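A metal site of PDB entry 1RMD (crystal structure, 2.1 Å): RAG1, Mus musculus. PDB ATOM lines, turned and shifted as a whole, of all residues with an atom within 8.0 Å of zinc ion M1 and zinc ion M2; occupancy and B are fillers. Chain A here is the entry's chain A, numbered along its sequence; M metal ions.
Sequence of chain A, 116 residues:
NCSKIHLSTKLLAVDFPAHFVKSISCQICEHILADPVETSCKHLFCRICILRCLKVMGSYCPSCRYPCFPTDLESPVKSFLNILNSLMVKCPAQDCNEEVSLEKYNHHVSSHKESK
OG of Ser 3 sits at hydrogen-bond distance from NE2 of His 31 (3.5 Å). SG of Cys 26 lies close to N of Ile 28 (3.4 Å). The backbone carbonyl oxygen of His 31 sits at hydrogen-bond distance from the backbone NH of Cys 26 (2.9 Å). The side-chain sulfur (SG) of Cys 46 sits close to the backbone NH (N) of Ala 34 (3.7 Å).
Of the 27 residues printed, 4 come within 4 Å of zinc ion M1. The nearest printed residue that does not touch zinc ion M1 is Cys 49 (4.4 Å).
Zinc ion M1 is bound by ND1 of His 6, ND1 of His 31, SG of Cys 2 and SG of Cys 29. Zinc ion M1 has four donor atoms within binding distance.
Zinc ion M2 is bound by SG of Cys 46 (2.2 Å), SG of Cys 49 (2.3 Å), SG of Cys 29 (2.3 Å) and SG of Cys 26 (2.3 Å).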
ATOM      1  N   ASN A   1     -20.348 -21.530   3.922  1.00  0.00           N
ATOM      2  CA  ASN A   1     -20.378 -21.288   5.404  1.00  0.00           C
ATOM      3  C   ASN A   1     -20.507 -19.808   5.782  1.00  0.00           C
ATOM      4  O   ASN A   1     -20.718 -18.943   4.909  1.00  0.00           O
ATOM      5  CB  ASN A   1     -19.118 -21.869   6.046  1.00  0.00           C
ATOM      6  CG  ASN A   1     -17.841 -21.466   5.338  1.00  0.00           C
ATOM      7  OD1 ASN A   1     -17.859 -20.658   4.408  1.00  0.00           O
ATOM      8  ND2 ASN A   1     -16.716 -22.024   5.775  1.00  0.00           N
ATOM      9  N   CYS A   2     -20.399 -19.512   7.077  1.00  0.00           N
ATOM     10  CA  CYS A   2     -20.483 -18.124   7.550  1.00  0.00           C
ATOM     11  C   CYS A   2     -19.215 -17.342   7.225  1.00  0.00           C
ATOM     12  O   CYS A   2     -19.118 -16.149   7.495  1.00  0.00           O
ATOM     13  CB  CYS A   2     -20.749 -18.073   9.066  1.00  0.00           C
ATOM     14  SG  CYS A   2     -19.569 -18.966  10.081  1.00  0.00           S
ATOM     15  N   SER A   3     -18.236 -18.040   6.656  1.00  0.00           N
ATOM     16  CA  SER A   3     -16.955 -17.456   6.261  1.00  0.00           C
ATOM     17  C   SER A   3     -17.180 -16.501   5.083  1.00  0.00           C
ATOM     18  O   SER A   3     -16.357 -15.621   4.821  1.00  0.00           O
ATOM     19  CB  SER A   3     -15.993 -18.581   5.857  1.00  0.00           C
ATOM     20  OG  SER A   3     -14.622 -18.206   5.995  1.00  0.00           O
ATOM     21  N   LYS A   4     -18.295 -16.700   4.371  1.00  0.00           N
ATOM     22  CA  LYS A   4     -18.669 -15.849   3.231  1.00  0.00           C
ATOM     23  C   LYS A   4     -19.208 -14.518   3.728  1.00  0.00           C
ATOM     24  O   LYS A   4     -19.245 -13.548   2.976  1.00  0.00           O
ATOM     25  CB  LYS A   4     -19.798 -16.499   2.420  1.00  0.00           C
ATOM     26  CG  LYS A   4     -19.365 -17.637   1.544  1.00  0.00           C
ATOM     27  CD  LYS A   4     -20.494 -18.106   0.664  1.00  0.00           C
ATOM     28  CE  LYS A   4     -19.962 -18.554  -0.658  1.00  0.00           C
ATOM     29  NZ  LYS A   4     -21.044 -19.117  -1.452  1.00  0.00           N
ATOM     30  N   ILE A   5     -19.659 -14.521   4.980  1.00  0.00           N
ATOM     31  CA  ILE A   5     -20.257 -13.345   5.601  1.00  0.00           C
ATOM     32  C   ILE A   5     -19.523 -12.813   6.827  1.00  0.00           C
ATOM     33  O   ILE A   5     -19.814 -11.685   7.279  1.00  0.00           O
ATOM     34  CB  ILE A   5     -21.732 -13.639   5.997  1.00  0.00           C
ATOM     35  CG1 ILE A   5     -21.862 -15.005   6.684  1.00  0.00           C
ATOM     36  CG2 ILE A   5     -22.633 -13.576   4.772  1.00  0.00           C
ATOM     37  CD1 ILE A   5     -23.232 -15.309   7.226  1.00  0.00           C
ATOM     38  N   HIS A   6     -18.597 -13.605   7.365  1.00  0.00           N
ATOM     39  CA  HIS A   6     -17.850 -13.223   8.554  1.00  0.00           C
ATOM     40  C   HIS A   6     -16.384 -12.882   8.304  1.00  0.00           C
ATOM     41  O   HIS A   6     -15.782 -13.351   7.349  1.00  0.00           O
ATOM     42  CB  HIS A   6     -17.957 -14.336   9.588  1.00  0.00           C
ATOM     43  CG  HIS A   6     -19.340 -14.489  10.166  1.00  0.00           C
ATOM     44  ND1 HIS A   6     -19.661 -15.567  10.968  1.00  0.00           N
ATOM     45  CD2 HIS A   6     -20.427 -13.705   9.990  1.00  0.00           C
ATOM     46  CE1 HIS A   6     -20.943 -15.410  11.251  1.00  0.00           C
ATOM     47  NE2 HIS A   6     -21.453 -14.301  10.684  1.00  0.00           N
ATOM     48  N   LEU A   7     -15.806 -12.037   9.163  1.00  0.00           N
ATOM     49  CA  LEU A   7     -14.411 -11.662   9.028  1.00  0.00           C
ATOM     50  C   LEU A   7     -13.486 -12.541   9.877  1.00  0.00           C
ATOM     51  O   LEU A   7     -13.821 -12.882  11.017  1.00  0.00           O
ATOM     52  CB  LEU A   7     -14.238 -10.189   9.394  1.00  0.00           C
ATOM     53  CG  LEU A   7     -13.773  -9.224   8.287  1.00  0.00           C
ATOM     54  CD1 LEU A   7     -14.521  -9.449   6.950  1.00  0.00           C
ATOM     55  CD2 LEU A   7     -13.962  -7.798   8.796  1.00  0.00           C
ATOM     56  N   SER A   8     -12.356 -12.948   9.304  1.00  0.00           N
ATOM     57  CA  SER A   8     -11.360 -13.771  10.004  1.00  0.00           C
ATOM     58  C   SER A   8     -10.541 -12.891  10.926  1.00  0.00           C
ATOM     59  O   SER A   8     -10.189 -11.753  10.564  1.00  0.00           O
ATOM     60  CB  SER A   8     -10.406 -14.434   9.003  1.00  0.00           C
ATOM     61  OG  SER A   8      -9.222 -14.877   9.661  1.00  0.00           O
ATOM     62  N   SER A  25     -13.940 -13.125  19.570  1.00  0.00           N
ATOM     63  CA  SER A  25     -14.287 -14.139  18.565  1.00  0.00           C
ATOM     64  C   SER A  25     -15.547 -14.970  18.919  1.00  0.00           C
ATOM     65  O   SER A  25     -15.884 -15.156  20.087  1.00  0.00           O
ATOM     66  CB  SER A  25     -13.099 -15.102  18.355  1.00  0.00           C
ATOM     67  OG  SER A  25     -11.907 -14.422  18.031  1.00  0.00           O
ATOM     68  N   CYS A  26     -16.252 -15.447  17.907  1.00  0.00           N
ATOM     69  CA  CYS A  26     -17.428 -16.275  18.113  1.00  0.00           C
ATOM     70  C   CYS A  26     -16.928 -17.648  18.563  1.00  0.00           C
ATOM     71  O   CYS A  26     -16.147 -18.280  17.874  1.00  0.00           O
ATOM     72  CB  CYS A  26     -18.211 -16.418  16.798  1.00  0.00           C
ATOM     73  SG  CYS A  26     -19.394 -17.749  16.831  1.00  0.00           S
ATOM     74  N   GLN A  27     -17.402 -18.107  19.715  1.00  0.00           N
ATOM     75  CA  GLN A  27     -16.945 -19.397  20.257  1.00  0.00           C
ATOM     76  C   GLN A  27     -17.325 -20.668  19.480  1.00  0.00           C
ATOM     77  O   GLN A  27     -16.851 -21.748  19.798  1.00  0.00           O
ATOM     78  CB  GLN A  27     -17.256 -19.521  21.750  1.00  0.00           C
ATOM     79  CG  GLN A  27     -16.546 -18.463  22.603  1.00  0.00           C
ATOM     80  CD  GLN A  27     -15.057 -18.355  22.310  1.00  0.00           C
ATOM     81  OE1 GLN A  27     -14.276 -19.218  22.686  1.00  0.00           O
ATOM     82  NE2 GLN A  27     -14.664 -17.290  21.638  1.00  0.00           N
ATOM     83  N   ILE A  28     -18.164 -20.492  18.456  1.00  0.00           N
ATOM     84  CA  ILE A  28     -18.561 -21.586  17.556  1.00  0.00           C
ATOM     85  C   ILE A  28     -17.767 -21.488  16.243  1.00  0.00           C
ATOM     86  O   ILE A  28     -16.908 -22.295  15.977  1.00  0.00           O
ATOM     87  CB  ILE A  28     -20.065 -21.530  17.234  1.00  0.00           C
ATOM     88  CG1 ILE A  28     -20.864 -22.023  18.441  1.00  0.00           C
ATOM     89  CG2 ILE A  28     -20.399 -22.398  16.013  1.00  0.00           C
ATOM     90  CD1 ILE A  28     -22.362 -21.761  18.346  1.00  0.00           C
ATOM     91  N   CYS A  29     -18.006 -20.439  15.470  1.00  0.00           N
ATOM     92  CA  CYS A  29     -17.351 -20.254  14.190  1.00  0.00           C
ATOM     93  C   CYS A  29     -15.937 -19.667  14.222  1.00  0.00           C
ATOM     94  O   CYS A  29     -15.219 -19.758  13.221  1.00  0.00           O
ATOM     95  CB  CYS A  29     -18.249 -19.435  13.241  1.00  0.00           C
ATOM     96  SG  CYS A  29     -18.348 -17.632  13.453  1.00  0.00           S
ATOM     97  N   GLU A  30     -15.525 -19.086  15.346  1.00  0.00           N
ATOM     98  CA  GLU A  30     -14.185 -18.495  15.487  1.00  0.00           C
ATOM     99  C   GLU A  30     -13.878 -17.210  14.702  1.00  0.00           C
ATOM    100  O   GLU A  30     -12.758 -16.709  14.710  1.00  0.00           O
ATOM    101  CB  GLU A  30     -13.099 -19.533  15.217  1.00  0.00           C
ATOM    102  CG  GLU A  30     -12.994 -20.523  16.346  1.00  0.00           C
ATOM    103  CD  GLU A  30     -11.916 -21.555  16.115  1.00  0.00           C
ATOM    104  OE1 GLU A  30     -10.859 -21.225  15.550  1.00  0.00           O
ATOM    105  OE2 GLU A  30     -12.140 -22.704  16.524  1.00  0.00           O
ATOM    106  N   HIS A  31     -14.874 -16.683  14.016  1.00  0.00           N
ATOM    107  CA  HIS A  31     -14.649 -15.442  13.274  1.00  0.00           C
ATOM    108  C   HIS A  31     -14.792 -14.274  14.253  1.00  0.00           C
ATOM    109  O   HIS A  31     -15.104 -14.498  15.442  1.00  0.00           O
ATOM    110  CB  HIS A  31     -15.691 -15.317  12.167  1.00  0.00           C
ATOM    111  CG  HIS A  31     -15.572 -16.373  11.114  1.00  0.00           C
ATOM    112  ND1 HIS A  31     -16.641 -17.166  10.789  1.00  0.00           N
ATOM    113  CD2 HIS A  31     -14.547 -16.619  10.269  1.00  0.00           C
ATOM    114  CE1 HIS A  31     -16.242 -17.875   9.749  1.00  0.00           C
ATOM    115  NE2 HIS A  31     -14.979 -17.565   9.402  1.00  0.00           N
ATOM    116  N   ILE A  32     -14.518 -13.053  13.802  1.00  0.00           N
ATOM    117  CA  ILE A  32     -14.745 -11.890  14.663  1.00  0.00           C
ATOM    118  C   ILE A  32     -16.278 -11.875  14.877  1.00  0.00           C
ATOM    119  O   ILE A  32     -17.052 -12.002  13.901  1.00  0.00           O
ATOM    120  CB  ILE A  32     -14.339 -10.567  13.985  1.00  0.00           C
ATOM    121  CG1 ILE A  32     -12.860 -10.595  13.638  1.00  0.00           C
ATOM    122  CG2 ILE A  32     -14.625  -9.400  14.916  1.00  0.00           C
ATOM    123  CD1 ILE A  32     -12.372  -9.344  12.905  1.00  0.00           C
ATOM    124  N   LEU A  33     -16.726 -11.778  16.124  1.00  0.00           N
ATOM    125  CA  LEU A  33     -18.179 -11.778  16.398  1.00  0.00           C
ATOM    126  C   LEU A  33     -18.981 -10.870  15.444  1.00  0.00           C
ATOM    127  O   LEU A  33     -18.645  -9.695  15.249  1.00  0.00           O
ATOM    128  CB  LEU A  33     -18.463 -11.313  17.837  1.00  0.00           C
ATOM    129  CG  LEU A  33     -18.057 -12.242  18.974  1.00  0.00           C
ATOM    130  CD1 LEU A  33     -17.817 -11.438  20.248  1.00  0.00           C
ATOM    131  CD2 LEU A  33     -19.111 -13.290  19.165  1.00  0.00           C
ATOM    132  N   ALA A  34     -20.032 -11.414  14.859  1.00  0.00           N
ATOM    133  CA  ALA A  34     -20.869 -10.620  13.978  1.00  0.00           C
ATOM    134  C   ALA A  34     -22.219 -10.658  14.658  1.00  0.00           C
ATOM    135  O   ALA A  34     -22.797 -11.725  14.769  1.00  0.00           O
ATOM    136  CB  ALA A  34     -20.944 -11.260  12.577  1.00  0.00           C
ATOM    137  N   ASP A  35     -22.704  -9.501  15.119  1.00  0.00           N
ATOM    138  CA  ASP A  35     -23.989  -9.394  15.842  1.00  0.00           C
ATOM    139  C   ASP A  35     -23.933 -10.307  17.052  1.00  0.00           C
ATOM    140  O   ASP A  35     -24.683 -11.285  17.147  1.00  0.00           O
ATOM    141  CB  ASP A  35     -25.159  -9.821  14.947  1.00  0.00           C
ATOM    142  CG  ASP A  35     -26.518  -9.417  15.497  1.00  0.00           C
ATOM    143  OD1 ASP A  35     -26.556  -8.579  16.423  1.00  0.00           O
ATOM    144  OD2 ASP A  35     -27.535  -9.934  15.007  1.00  0.00           O
ATOM    145  N   LEU A  44     -19.881 -15.606  24.445  1.00  0.00           N
ATOM    146  CA  LEU A  44     -20.286 -14.942  23.205  1.00  0.00           C
ATOM    147  C   LEU A  44     -20.334 -15.770  21.910  1.00  0.00           C
ATOM    148  O   LEU A  44     -19.490 -16.648  21.692  1.00  0.00           O
ATOM    149  CB  LEU A  44     -19.402 -13.706  22.993  1.00  0.00           C
ATOM    150  CG  LEU A  44     -19.383 -12.699  24.152  1.00  0.00           C
ATOM    151  CD1 LEU A  44     -18.540 -11.528  23.809  1.00  0.00           C
ATOM    152  CD2 LEU A  44     -20.798 -12.244  24.487  1.00  0.00           C
ATOM    153  N   PHE A  45     -21.329 -15.500  21.067  1.00  0.00           N
ATOM    154  CA  PHE A  45     -21.520 -16.180  19.763  1.00  0.00           C
ATOM    155  C   PHE A  45     -22.285 -15.239  18.833  1.00  0.00           C
ATOM    156  O   PHE A  45     -23.098 -14.433  19.294  1.00  0.00           O
ATOM    157  CB  PHE A  45     -22.369 -17.455  19.885  1.00  0.00           C
ATOM    158  CG  PHE A  45     -21.955 -18.355  20.977  1.00  0.00           C
ATOM    159  CD1 PHE A  45     -22.459 -18.184  22.264  1.00  0.00           C
ATOM    160  CD2 PHE A  45     -21.013 -19.353  20.756  1.00  0.00           C
ATOM    161  CE1 PHE A  45     -22.029 -18.982  23.324  1.00  0.00           C
ATOM    162  CE2 PHE A  45     -20.570 -20.169  21.811  1.00  0.00           C
ATOM    163  CZ  PHE A  45     -21.094 -19.971  23.111  1.00  0.00           C
ATOM    164  N   CYS A  46     -22.043 -15.350  17.516  1.00  0.00           N
ATOM    165  CA  CYS A  46     -22.773 -14.538  16.530  1.00  0.00           C
ATOM    166  C   CYS A  46     -24.217 -15.002  16.690  1.00  0.00           C
ATOM    167  O   CYS A  46     -24.442 -16.204  16.829  1.00  0.00           O
ATOM    168  CB  CYS A  46     -22.349 -14.870  15.087  1.00  0.00           C
ATOM    169  SG  CYS A  46     -20.574 -15.031  14.695  1.00  0.00           S
ATOM    170  N   ARG A  47     -25.185 -14.077  16.670  1.00  0.00           N
ATOM    171  CA  ARG A  47     -26.611 -14.441  16.788  1.00  0.00           C
ATOM    172  C   ARG A  47     -27.018 -15.665  15.937  1.00  0.00           C
ATOM    173  O   ARG A  47     -27.752 -16.507  16.426  1.00  0.00           O
ATOM    174  CB  ARG A  47     -27.503 -13.248  16.392  1.00  0.00           C
ATOM    175  CG  ARG A  47     -29.001 -13.558  16.178  1.00  0.00           C
ATOM    176  CD  ARG A  47     -29.850 -13.419  17.444  1.00  0.00           C
ATOM    177  NE  ARG A  47     -29.688 -12.145  18.147  1.00  0.00           N
ATOM    178  CZ  ARG A  47     -29.647 -10.960  17.563  1.00  0.00           C
ATOM    179  NH1 ARG A  47     -29.775 -10.864  16.246  1.00  0.00           N
ATOM    180  NH2 ARG A  47     -29.407  -9.865  18.278  1.00  0.00           N
ATOM    181  N   ILE A  48     -26.533 -15.782  14.710  1.00  0.00           N
ATOM    182  CA  ILE A  48     -26.923 -16.931  13.902  1.00  0.00           C
ATOM    183  C   ILE A  48     -26.209 -18.216  14.277  1.00  0.00           C
ATOM    184  O   ILE A  48     -26.792 -19.300  14.164  1.00  0.00           O
ATOM    185  CB  ILE A  48     -26.728 -16.726  12.364  1.00  0.00           C
ATOM    186  CG1 ILE A  48     -25.247 -16.617  12.007  1.00  0.00           C
ATOM    187  CG2 ILE A  48     -27.526 -15.517  11.880  1.00  0.00           C
ATOM    188  CD1 ILE A  48     -24.957 -16.549  10.498  1.00  0.00           C
ATOM    189  N   CYS A  49     -24.974 -18.120  14.730  1.00  0.00           N
ATOM    190  CA  CYS A  49     -24.246 -19.349  15.048  1.00  0.00           C
ATOM    191  C   CYS A  49     -24.845 -20.069  16.246  1.00  0.00           C
ATOM    192  O   CYS A  49     -25.044 -21.303  16.209  1.00  0.00           O
ATOM    193  CB  CYS A  49     -22.766 -19.066  15.262  1.00  0.00           C
ATOM    194  SG  CYS A  49     -21.952 -18.405  13.775  1.00  0.00           S
ATOM    195  N   ILE A  50     -25.196 -19.305  17.277  1.00  0.00           N
ATOM    196  CA  ILE A  50     -25.746 -19.888  18.484  1.00  0.00           C
ATOM    197  C   ILE A  50     -27.162 -20.470  18.297  1.00  0.00           C
ATOM    198  O   ILE A  50     -27.410 -21.617  18.680  1.00  0.00           O
ATOM    199  CB  ILE A  50     -25.655 -18.884  19.678  1.00  0.00           C
ATOM    200  CG1 ILE A  50     -26.080 -19.582  20.968  1.00  0.00           C
ATOM    201  CG2 ILE A  50     -26.440 -17.613  19.384  1.00  0.00           C
ATOM    202  CD1 ILE A  50     -25.268 -20.826  21.295  1.00  0.00           C
ATOM    203  N   ARG A  52     -28.469 -21.726  15.709  1.00  0.00           N
ATOM    204  CA  ARG A  52     -28.463 -22.972  14.962  1.00  0.00           C
ATOM    205  C   ARG A  52     -28.007 -24.113  15.853  1.00  0.00           C
ATOM    206  O   ARG A  52     -28.559 -25.211  15.789  1.00  0.00           O
ATOM    207  CB  ARG A  52     -27.589 -22.853  13.704  1.00  0.00           C
ATOM    208  CG  ARG A  52     -27.472 -24.138  12.860  1.00  0.00           C
ATOM    209  CD  ARG A  52     -26.298 -25.040  13.288  1.00  0.00           C
ATOM    210  NE  ARG A  52     -25.080 -24.255  13.529  1.00  0.00           N
ATOM    211  CZ  ARG A  52     -23.939 -24.723  14.029  1.00  0.00           C
ATOM    212  NH1 ARG A  52     -23.810 -26.011  14.363  1.00  0.00           N
ATOM    213  NH2 ARG A  52     -22.939 -23.894  14.293  1.00  0.00           N
HETATM  214 ZN    ZN M   1     -18.679 -17.138  11.181  1.00  0.00          ZN
HETATM  215 ZN    ZN M   2     -20.250 -17.246  14.724  1.00  0.00          ZN
